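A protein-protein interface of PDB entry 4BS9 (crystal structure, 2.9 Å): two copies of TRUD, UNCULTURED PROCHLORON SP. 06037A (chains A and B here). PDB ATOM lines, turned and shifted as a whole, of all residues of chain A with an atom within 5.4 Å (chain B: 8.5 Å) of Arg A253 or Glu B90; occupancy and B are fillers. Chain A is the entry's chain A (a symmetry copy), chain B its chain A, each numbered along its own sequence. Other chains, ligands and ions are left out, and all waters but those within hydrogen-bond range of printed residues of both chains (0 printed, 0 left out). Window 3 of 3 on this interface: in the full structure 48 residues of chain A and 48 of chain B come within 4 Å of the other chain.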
ATOM      1  N   ASP A 165      33.945   6.345  17.059  1.00  0.00           N
ATOM      2  CA  ASP A 165      32.849   5.850  16.216  1.00  0.00           C
ATOM      3  C   ASP A 165      32.962   6.348  14.768  1.00  0.00           C
ATOM      4  O   ASP A 165      32.181   5.934  13.905  1.00  0.00           O
ATOM      5  CB  ASP A 165      31.477   6.192  16.811  1.00  0.00           C
ATOM      6  CG  ASP A 165      31.121   7.661  16.686  1.00  0.00           C
ATOM      7  OD1 ASP A 165      31.966   8.513  17.045  1.00  0.00           O
ATOM      8  OD2 ASP A 165      29.981   7.962  16.254  1.00  0.00           O
ATOM      9  N   ASP A 166      33.938   7.215  14.500  1.00  0.00           N
ATOM     10  CA  ASP A 166      34.207   7.675  13.141  1.00  0.00           C
ATOM     11  C   ASP A 166      35.616   8.235  12.959  1.00  0.00           C
ATOM     12  O   ASP A 166      36.096   9.015  13.757  1.00  0.00           O
ATOM     13  CB  ASP A 166      33.191   8.722  12.727  1.00  0.00           C
ATOM     14  CG  ASP A 166      33.276   9.048  11.266  1.00  0.00           C
ATOM     15  OD1 ASP A 166      32.861   8.197  10.444  1.00  0.00           O
ATOM     16  OD2 ASP A 166      33.755  10.160  10.949  1.00  0.00           O
ATOM     17  N   LYS A 190      37.660   1.484  15.709  1.00  0.00           N
ATOM     18  CA  LYS A 190      36.215   1.644  15.712  1.00  0.00           C
ATOM     19  C   LYS A 190      35.600   0.290  15.990  1.00  0.00           C
ATOM     20  O   LYS A 190      35.500  -0.533  15.087  1.00  0.00           O
ATOM     21  CB  LYS A 190      35.710   2.158  14.373  1.00  0.00           C
ATOM     22  CG  LYS A 190      34.221   2.436  14.375  1.00  0.00           C
ATOM     23  CD  LYS A 190      33.737   3.052  13.064  1.00  0.00           C
ATOM     24  CE  LYS A 190      33.399   1.986  12.037  1.00  0.00           C
ATOM     25  NZ  LYS A 190      32.103   1.267  12.289  1.00  0.00           N
ATOM     26  N   VAL A 192      32.458  -0.019  17.368  1.00  0.00           N
ATOM     27  CA  VAL A 192      31.007   0.072  17.196  1.00  0.00           C
ATOM     28  C   VAL A 192      30.631   0.022  15.714  1.00  0.00           C
ATOM     29  O   VAL A 192      31.480   0.200  14.831  1.00  0.00           O
ATOM     30  CB  VAL A 192      30.440   1.336  17.854  1.00  0.00           C
ATOM     31  CG1 VAL A 192      30.567   1.225  19.353  1.00  0.00           C
ATOM     32  CG2 VAL A 192      31.153   2.594  17.395  1.00  0.00           C
ATOM     33  N   GLY A 193      29.363  -0.232  15.430  1.00  0.00           N
ATOM     34  CA  GLY A 193      28.947  -0.388  14.040  1.00  0.00           C
ATOM     35  C   GLY A 193      29.033  -1.809  13.487  1.00  0.00           C
ATOM     36  O   GLY A 193      29.628  -2.705  14.081  1.00  0.00           O
ATOM     37  N   THR A 251      26.648  10.881  13.232  1.00  0.00           N
ATOM     38  CA  THR A 251      26.218   9.540  12.738  1.00  0.00           C
ATOM     39  C   THR A 251      25.440   8.557  13.706  1.00  0.00           C
ATOM     40  O   THR A 251      25.376   8.783  14.916  1.00  0.00           O
ATOM     41  CB  THR A 251      27.480   8.824  12.145  1.00  0.00           C
ATOM     42  OG1 THR A 251      27.119   7.558  11.582  1.00  0.00           O
ATOM     43  CG2 THR A 251      28.583   8.628  13.205  1.00  0.00           C
ATOM     44  N   ALA A 252      24.841   7.492  13.137  1.00  0.00           N
ATOM     45  CA  ALA A 252      24.176   6.382  13.889  1.00  0.00           C
ATOM     46  C   ALA A 252      24.964   5.045  13.755  1.00  0.00           C
ATOM     47  O   ALA A 252      25.770   4.877  12.820  1.00  0.00           O
ATOM     48  CB  ALA A 252      22.727   6.204  13.431  1.00  0.00           C
ATOM     49  N   ARG A 253      24.744   4.096  14.678  1.00  0.00           N
ATOM     50  CA  ARG A 253      25.625   2.910  14.770  1.00  0.00           C
ATOM     51  C   ARG A 253      25.000   1.618  15.302  1.00  0.00           C
ATOM     52  O   ARG A 253      24.575   1.548  16.452  1.00  0.00           O
ATOM     53  CB  ARG A 253      26.851   3.228  15.639  1.00  0.00           C
ATOM     54  CG  ARG A 253      27.877   4.147  14.994  1.00  0.00           C
ATOM     55  CD  ARG A 253      28.506   3.523  13.757  1.00  0.00           C
ATOM     56  NE  ARG A 253      29.356   4.463  13.020  1.00  0.00           N
ATOM     57  CZ  ARG A 253      29.014   5.104  11.901  1.00  0.00           C
ATOM     58  NH1 ARG A 253      27.810   4.935  11.343  1.00  0.00           N
ATOM     59  NH2 ARG A 253      29.893   5.937  11.337  1.00  0.00           N
ATOM     60  N   ALA A 254      25.008   0.585  14.467  1.00  0.00           N
ATOM     61  CA  ALA A 254      24.559  -0.746  14.863  1.00  0.00           C
ATOM     62  C   ALA A 254      25.611  -1.473  15.684  1.00  0.00           C
ATOM     63  O   ALA A 254      26.770  -1.514  15.306  1.00  0.00           O
ATOM     64  CB  ALA A 254      24.256  -1.574  13.635  1.00  0.00           C
ATOM     65  N   THR A 255      25.202  -2.083  16.785  1.00  0.00           N
ATOM     66  CA  THR A 255      26.151  -2.685  17.713  1.00  0.00           C
ATOM     67  C   THR A 255      25.417  -3.742  18.544  1.00  0.00           C
ATOM     68  O   THR A 255      24.508  -3.419  19.319  1.00  0.00           O
ATOM     69  CB  THR A 255      26.797  -1.608  18.650  1.00  0.00           C
ATOM     70  OG1 THR A 255      27.230  -0.470  17.890  1.00  0.00           O
ATOM     71  CG2 THR A 255      28.006  -2.150  19.425  1.00  0.00           C
ATOM     72  N   LEU A 256      25.787  -5.008  18.362  1.00  0.00           N
ATOM     73  CA  LEU A 256      25.428  -6.025  19.334  1.00  0.00           C
ATOM     74  C   LEU A 256      26.548  -6.056  20.355  1.00  0.00           C
ATOM     75  O   LEU A 256      27.679  -5.716  20.031  1.00  0.00           O
ATOM     76  CB  LEU A 256      25.335  -7.396  18.702  1.00  0.00           C
ATOM     77  CG  LEU A 256      24.461  -7.561  17.482  1.00  0.00           C
ATOM     78  CD1 LEU A 256      24.528  -9.007  17.045  1.00  0.00           C
ATOM     79  CD2 LEU A 256      23.038  -7.177  17.800  1.00  0.00           C
ATOM     80  N   PRO B  10      16.493   2.086  12.284  1.00  0.00           N
ATOM     81  CA  PRO B  10      17.415   2.666  13.250  1.00  0.00           C
ATOM     82  C   PRO B  10      18.865   2.675  12.796  1.00  0.00           C
ATOM     83  O   PRO B  10      19.675   3.312  13.443  1.00  0.00           O
ATOM     84  CB  PRO B  10      17.232   1.797  14.501  1.00  0.00           C
ATOM     85  CG  PRO B  10      16.604   0.537  14.028  1.00  0.00           C
ATOM     86  CD  PRO B  10      15.846   0.858  12.777  1.00  0.00           C
ATOM     87  N   HIS B  11      19.197   2.007  11.694  1.00  0.00           N
ATOM     88  CA  HIS B  11      20.565   2.058  11.202  1.00  0.00           C
ATOM     89  C   HIS B  11      20.817   3.253  10.315  1.00  0.00           C
ATOM     90  O   HIS B  11      21.942   3.445   9.871  1.00  0.00           O
ATOM     91  CB  HIS B  11      20.992   0.756  10.507  1.00  0.00           C
ATOM     92  CG  HIS B  11      20.395   0.546   9.158  1.00  0.00           C
ATOM     93  ND1 HIS B  11      19.198  -0.104   8.972  1.00  0.00           N
ATOM     94  CD2 HIS B  11      20.850   0.851   7.925  1.00  0.00           C
ATOM     95  CE1 HIS B  11      18.926  -0.169   7.682  1.00  0.00           C
ATOM     96  NE2 HIS B  11      19.914   0.403   7.024  1.00  0.00           N
ATOM     97  N   PHE B  12      19.781   4.057  10.071  1.00  0.00           N
ATOM     98  CA  PHE B  12      19.923   5.300   9.317  1.00  0.00           C
ATOM     99  C   PHE B  12      19.970   6.497  10.255  1.00  0.00           C
ATOM    100  O   PHE B  12      19.164   6.606  11.174  1.00  0.00           O
ATOM    101  CB  PHE B  12      18.763   5.479   8.335  1.00  0.00           C
ATOM    102  CG  PHE B  12      18.827   4.577   7.138  1.00  0.00           C
ATOM    103  CD1 PHE B  12      19.968   4.524   6.350  1.00  0.00           C
ATOM    104  CD2 PHE B  12      17.742   3.792   6.789  1.00  0.00           C
ATOM    105  CE1 PHE B  12      20.021   3.699   5.239  1.00  0.00           C
ATOM    106  CE2 PHE B  12      17.787   2.971   5.678  1.00  0.00           C
ATOM    107  CZ  PHE B  12      18.925   2.926   4.898  1.00  0.00           C
ATOM    108  N   HIS B  13      20.941   7.379  10.031  1.00  0.00           N
ATOM    109  CA  HIS B  13      20.914   8.716  10.611  1.00  0.00           C
ATOM    110  C   HIS B  13      20.168   9.636   9.645  1.00  0.00           C
ATOM    111  O   HIS B  13      20.634   9.921   8.544  1.00  0.00           O
ATOM    112  CB  HIS B  13      22.317   9.268  10.889  1.00  0.00           C
ATOM    113  CG  HIS B  13      22.311  10.715  11.283  1.00  0.00           C
ATOM    114  ND1 HIS B  13      21.547  11.198  12.327  1.00  0.00           N
ATOM    115  CD2 HIS B  13      22.940  11.791  10.752  1.00  0.00           C
ATOM    116  CE1 HIS B  13      21.714  12.505  12.429  1.00  0.00           C
ATOM    117  NE2 HIS B  13      22.557  12.889  11.488  1.00  0.00           N
ATOM    118  N   LEU B  25      21.426   8.367   6.155  1.00  0.00           N
ATOM    119  CA  LEU B  25      22.842   8.050   6.149  1.00  0.00           C
ATOM    120  C   LEU B  25      23.100   6.811   6.984  1.00  0.00           C
ATOM    121  O   LEU B  25      22.784   6.772   8.165  1.00  0.00           O
ATOM    122  CB  LEU B  25      23.643   9.233   6.671  1.00  0.00           C
ATOM    123  CG  LEU B  25      23.361  10.534   5.917  1.00  0.00           C
ATOM    124  CD1 LEU B  25      23.955  11.700   6.685  1.00  0.00           C
ATOM    125  CD2 LEU B  25      23.916  10.480   4.505  1.00  0.00           C
ATOM    126  N   GLY B  26      23.664   5.793   6.349  1.00  0.00           N
ATOM    127  CA  GLY B  26      23.993   4.548   7.017  1.00  0.00           C
ATOM    128  C   GLY B  26      25.383   4.101   6.633  1.00  0.00           C
ATOM    129  O   GLY B  26      25.838   4.368   5.526  1.00  0.00           O
ATOM    130  N   GLU B  27      26.053   3.394   7.536  1.00  0.00           N
ATOM    131  CA  GLU B  27      27.456   3.081   7.327  1.00  0.00           C
ATOM    132  C   GLU B  27      27.706   2.114   6.164  1.00  0.00           C
ATOM    133  O   GLU B  27      28.822   2.048   5.663  1.00  0.00           O
ATOM    134  CB  GLU B  27      28.142   2.638   8.629  1.00  0.00           C
ATOM    135  CG  GLU B  27      27.977   1.196   9.081  1.00  0.00           C
ATOM    136  CD  GLU B  27      28.799   0.913  10.344  1.00  0.00           C
ATOM    137  OE1 GLU B  27      30.025   0.627  10.239  1.00  0.00           O
ATOM    138  OE2 GLU B  27      28.212   0.989  11.447  1.00  0.00           O
ATOM    139  N   GLN B  28      26.680   1.400   5.708  1.00  0.00           N
ATOM    140  CA  GLN B  28      26.817   0.518   4.537  1.00  0.00           C
ATOM    141  C   GLN B  28      25.897   0.949   3.376  1.00  0.00           C
ATOM    142  O   GLN B  28      25.465   0.114   2.573  1.00  0.00           O
ATOM    143  CB  GLN B  28      26.518  -0.940   4.923  1.00  0.00           C
ATOM    144  CG  GLN B  28      27.254  -1.430   6.158  1.00  0.00           C
ATOM    145  CD  GLN B  28      27.574  -2.917   6.122  1.00  0.00           C
ATOM    146  OE1 GLN B  28      27.784  -3.487   5.055  1.00  0.00           O
ATOM    147  NE2 GLN B  28      27.645  -3.545   7.296  1.00  0.00           N
ATOM    148  N   ASN B  30      23.860   4.925   1.698  1.00  0.00           N
ATOM    149  CA  ASN B  30      23.072   6.151   1.836  1.00  0.00           C
ATOM    150  C   ASN B  30      21.888   6.200   0.863  1.00  0.00           C
ATOM    151  O   ASN B  30      21.820   5.454  -0.115  1.00  0.00           O
ATOM    152  CB  ASN B  30      23.957   7.360   1.584  1.00  0.00           C
ATOM    153  CG  ASN B  30      25.113   7.456   2.567  1.00  0.00           C
ATOM    154  OD1 ASN B  30      24.979   7.075   3.734  1.00  0.00           O
ATOM    155  ND2 ASN B  30      26.256   7.978   2.103  1.00  0.00           N
ATOM    156  N   LEU B  87      14.475  -3.672  22.777  1.00  0.00           N
ATOM    157  CA  LEU B  87      15.816  -3.684  22.179  1.00  0.00           C
ATOM    158  C   LEU B  87      16.454  -2.298  22.215  1.00  0.00           C
ATOM    159  O   LEU B  87      15.765  -1.321  22.058  1.00  0.00           O
ATOM    160  CB  LEU B  87      15.734  -4.109  20.711  1.00  0.00           C
ATOM    161  CG  LEU B  87      15.223  -5.498  20.360  1.00  0.00           C
ATOM    162  CD1 LEU B  87      15.112  -5.646  18.858  1.00  0.00           C
ATOM    163  CD2 LEU B  87      16.159  -6.563  20.883  1.00  0.00           C
ATOM    164  N   SER B  88      17.772  -2.223  22.398  1.00  0.00           N
ATOM    165  CA  SER B  88      18.537  -1.008  22.127  1.00  0.00           C
ATOM    166  C   SER B  88      18.233  -0.536  20.729  1.00  0.00           C
ATOM    167  O   SER B  88      17.914  -1.353  19.863  1.00  0.00           O
ATOM    168  CB  SER B  88      20.033  -1.313  22.124  1.00  0.00           C
ATOM    169  OG  SER B  88      20.572  -1.505  23.408  1.00  0.00           O
ATOM    170  N   LEU B  89      18.399   0.759  20.478  1.00  0.00           N
ATOM    171  CA  LEU B  89      18.524   1.236  19.093  1.00  0.00           C
ATOM    172  C   LEU B  89      19.779   0.642  18.457  1.00  0.00           C
ATOM    173  O   LEU B  89      19.736   0.180  17.317  1.00  0.00           O
ATOM    174  CB  LEU B  89      18.523   2.766  19.009  1.00  0.00           C
ATOM    175  CG  LEU B  89      17.167   3.361  18.608  1.00  0.00           C
ATOM    176  CD1 LEU B  89      15.980   2.694  19.305  1.00  0.00           C
ATOM    177  CD2 LEU B  89      17.172   4.854  18.882  1.00  0.00           C
ATOM    178  N   GLU B  90      20.873   0.622  19.222  1.00  0.00           N
ATOM    179  CA  GLU B  90      22.133  -0.035  18.822  1.00  0.00           C
ATOM    180  C   GLU B  90      21.853  -1.394  18.218  1.00  0.00           C
ATOM    181  O   GLU B  90      22.309  -1.705  17.127  1.00  0.00           O
ATOM    182  CB  GLU B  90      23.061  -0.230  20.030  1.00  0.00           C
ATOM    183  CG  GLU B  90      23.943   0.954  20.357  1.00  0.00           C
ATOM    184  CD  GLU B  90      23.217   2.075  21.077  1.00  0.00           C
ATOM    185  OE1 GLU B  90      21.962   2.135  21.056  1.00  0.00           O
ATOM    186  OE2 GLU B  90      23.919   2.920  21.674  1.00  0.00           O
ATOM    187  N   VAL B  91      21.081  -2.189  18.953  1.00  0.00           N
ATOM    188  CA  VAL B  91      20.792  -3.564  18.579  1.00  0.00           C
ATOM    189  C   VAL B  91      19.781  -3.621  17.463  1.00  0.00           C
ATOM    190  O   VAL B  91      19.961  -4.378  16.512  1.00  0.00           O
ATOM    191  CB  VAL B  91      20.253  -4.368  19.776  1.00  0.00           C
ATOM    192  CG1 VAL B  91      19.709  -5.725  19.325  1.00  0.00           C
ATOM    193  CG2 VAL B  91      21.354  -4.536  20.806  1.00  0.00           C
ATOM    194  N   ALA B  92      18.712  -2.841  17.591  1.00  0.00           N
ATOM    195  CA  ALA B  92      17.705  -2.792  16.544  1.00  0.00           C
ATOM    196  C   ALA B  92      18.396  -2.478  15.220  1.00  0.00           C
ATOM    197  O   ALA B  92      18.156  -3.146  14.213  1.00  0.00           O
ATOM    198  CB  ALA B  92      16.643  -1.757  16.863  1.00  0.00           C
ATOM    199  N   ALA B  93      19.300  -1.504  15.256  1.00  0.00           N
ATOM    200  CA  ALA B  93      20.042  -1.081  14.069  1.00  0.00           C
ATOM    201  C   ALA B  93      20.784  -2.211  13.387  1.00  0.00           C
ATOM    202  O   ALA B  93      20.902  -2.218  12.167  1.00  0.00           O
ATOM    203  CB  ALA B  93      21.023   0.011  14.422  1.00  0.00           C
ATOM    204  N   PHE B  94      21.291  -3.159  14.164  1.00  0.00           N
ATOM    205  CA  PHE B  94      22.086  -4.234  13.597  1.00  0.00           C
ATOM    206  C   PHE B  94      21.223  -5.097  12.734  1.00  0.00           C
ATOM    207  O   PHE B  94      21.592  -5.455  11.609  1.00  0.00           O
ATOM    208  CB  PHE B  94      22.715  -5.103  14.683  1.00  0.00           C
ATOM    209  CG  PHE B  94      23.511  -6.238  14.128  1.00  0.00           C
ATOM    210  CD1 PHE B  94      24.782  -6.018  13.637  1.00  0.00           C
ATOM    211  CD2 PHE B  94      22.963  -7.507  14.035  1.00  0.00           C
ATOM    212  CE1 PHE B  94      25.519  -7.044  13.096  1.00  0.00           C
ATOM    213  CE2 PHE B  94      23.693  -8.551  13.497  1.00  0.00           C
ATOM    214  CZ  PHE B  94      24.977  -8.320  13.030  1.00  0.00           C
ATOM    215  N   TRP B  95      20.072  -5.439  13.301  1.00  0.00           N
ATOM    216  CA  TRP B  95      19.129  -6.321  12.659  1.00  0.00           C
ATOM    217  C   TRP B  95      18.480  -5.623  11.481  1.00  0.00           C
ATOM    218  O   TRP B  95      18.187  -6.273  10.478  1.00  0.00           O
ATOM    219  CB  TRP B  95      18.098  -6.805  13.669  1.00  0.00           C
ATOM    220  CG  TRP B  95      18.747  -7.617  14.736  1.00  0.00           C
ATOM    221  CD1 TRP B  95      18.956  -7.253  16.021  1.00  0.00           C
ATOM    222  CD2 TRP B  95      19.325  -8.912  14.587  1.00  0.00           C
ATOM    223  NE1 TRP B  95      19.605  -8.248  16.695  1.00  0.00           N
ATOM    224  CE2 TRP B  95      19.854  -9.276  15.832  1.00  0.00           C
ATOM    225  CE3 TRP B  95      19.453  -9.794  13.517  1.00  0.00           C
ATOM    226  CZ2 TRP B  95      20.500 -10.490  16.043  1.00  0.00           C
ATOM    227  CZ3 TRP B  95      20.075 -10.992  13.722  1.00  0.00           C
ATOM    228  CH2 TRP B  95      20.594 -11.338  14.978  1.00  0.00           C
ATOM    229  N   SER B  96      18.273  -4.307  11.575  1.00  0.00           N
ATOM    230  CA  SER B  96      17.745  -3.558  10.436  1.00  0.00           C
ATOM    231  C   SER B  96      18.818  -3.373   9.359  1.00  0.00           C
ATOM    232  O   SER B  96      18.499  -3.438   8.165  1.00  0.00           O
ATOM    233  CB  SER B  96      17.159  -2.212  10.854  1.00  0.00           C
ATOM    234  OG  SER B  96      18.167  -1.374  11.350  1.00  0.00           O
ATOM    235  N   GLU B  97      20.077  -3.170   9.758  1.00  0.00           N
ATOM    236  CA  GLU B  97      21.172  -3.142   8.777  1.00  0.00           C
ATOM    237  C   GLU B  97      21.212  -4.479   8.016  1.00  0.00           C
ATOM    238  O   GLU B  97      21.664  -4.522   6.892  1.00  0.00           O
ATOM    239  CB  GLU B  97      22.543  -2.824   9.426  1.00  0.00           C
ATOM    240  CG  GLU B  97      23.729  -2.639   8.457  1.00  0.00           C
ATOM    241  CD  GLU B  97      24.270  -1.206   8.390  1.00  0.00           C
ATOM    242  OE1 GLU B  97      24.941  -0.780   9.355  1.00  0.00           O
ATOM    243  OE2 GLU B  97      24.055  -0.496   7.371  1.00  0.00           O
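The side-chain amino group (NZ) of Lys A190 is in salt-bridge range of the side-chain carboxylate (OE1) of Glu B27 (3.0 Å). The side-chain carboxylate of Glu B27 lies within salt-bridge range of the guanidinium group of Arg A253 (3.97 Å). The backbone carbonyl oxygen (O) of Glu B90 is in hydrogen-bond range of the backbone NH (N) of Thr A255, at 2.9 Å.
N of His B13 is in hydrogen-bond range of O of Leu B25, at 2.7 Å. The backbone carbonyl oxygen (O) of Ala B93 lies within hydrogen-bond range of the side-chain hydroxyl (OG) of Ser B96 (3.0 Å). O of Asp A165 is in hydrogen-bond range of NE of Arg A253. OD1 of Asp A166 lies within salt-bridge range of NH2 of Arg A253 (3.8 Å). The side-chain amino group (NZ) of Lys A190 lies within hydrogen-bond range of the backbone carbonyl oxygen (O) of Val A192 (2.8 Å). OG1 of Thr A251 is in hydrogen-bond range of NH1 of Arg A253 (2.7 Å).
CA of Gly A193 touches OE2 of Glu B27 (3.0 Å). Ala A252 touches His B13. O of Arg A253 touches CA of Glu B90, at 3.8 Å. Glu B90 touches Ala A254. CB of Ala A254 touches C of Ala B93, at 3.5 Å. CB of Ala A254 touches N of Phe B94, at 3.4 Å. N of Val B91 touches O of Thr A255, at 3.7 Å. Leu A256 touches Val B91 (CD2 to CG1, 3.9 Å). Leu A256 touches Phe B94. Leu A256 touches Trp B95 (CD2 to NE1, 3.8 Å).
Glu B90 touches just these residues of chain A: Arg A253, Ala A254 and Thr A255. Of the printed residues of chain B, Ala A254 touches Glu B90 (3.3 Å), Ala B93 (3.5 Å) and Phe B94 (3.4 Å). Of the printed residues of chain A, His B13 touches Ala A252. Of the printed residues of chain B, Lys A190 touches Glu B27 (3.0 Å). Of the printed residues of chain A, Phe B94 touches Ala A254 and Leu A256. The nearest residue of chain A that does not touch Glu B90 is Leu A256 (5.0 Å).
Hydrophobic or aromatic side chains of chain B within 4 Å of the printed part of chain A: His B13, Val B91, Ala B93, Phe B94 and Trp B95. Among the printed residues, 13 pairs touch across the chains.
No position is printed for both chains.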
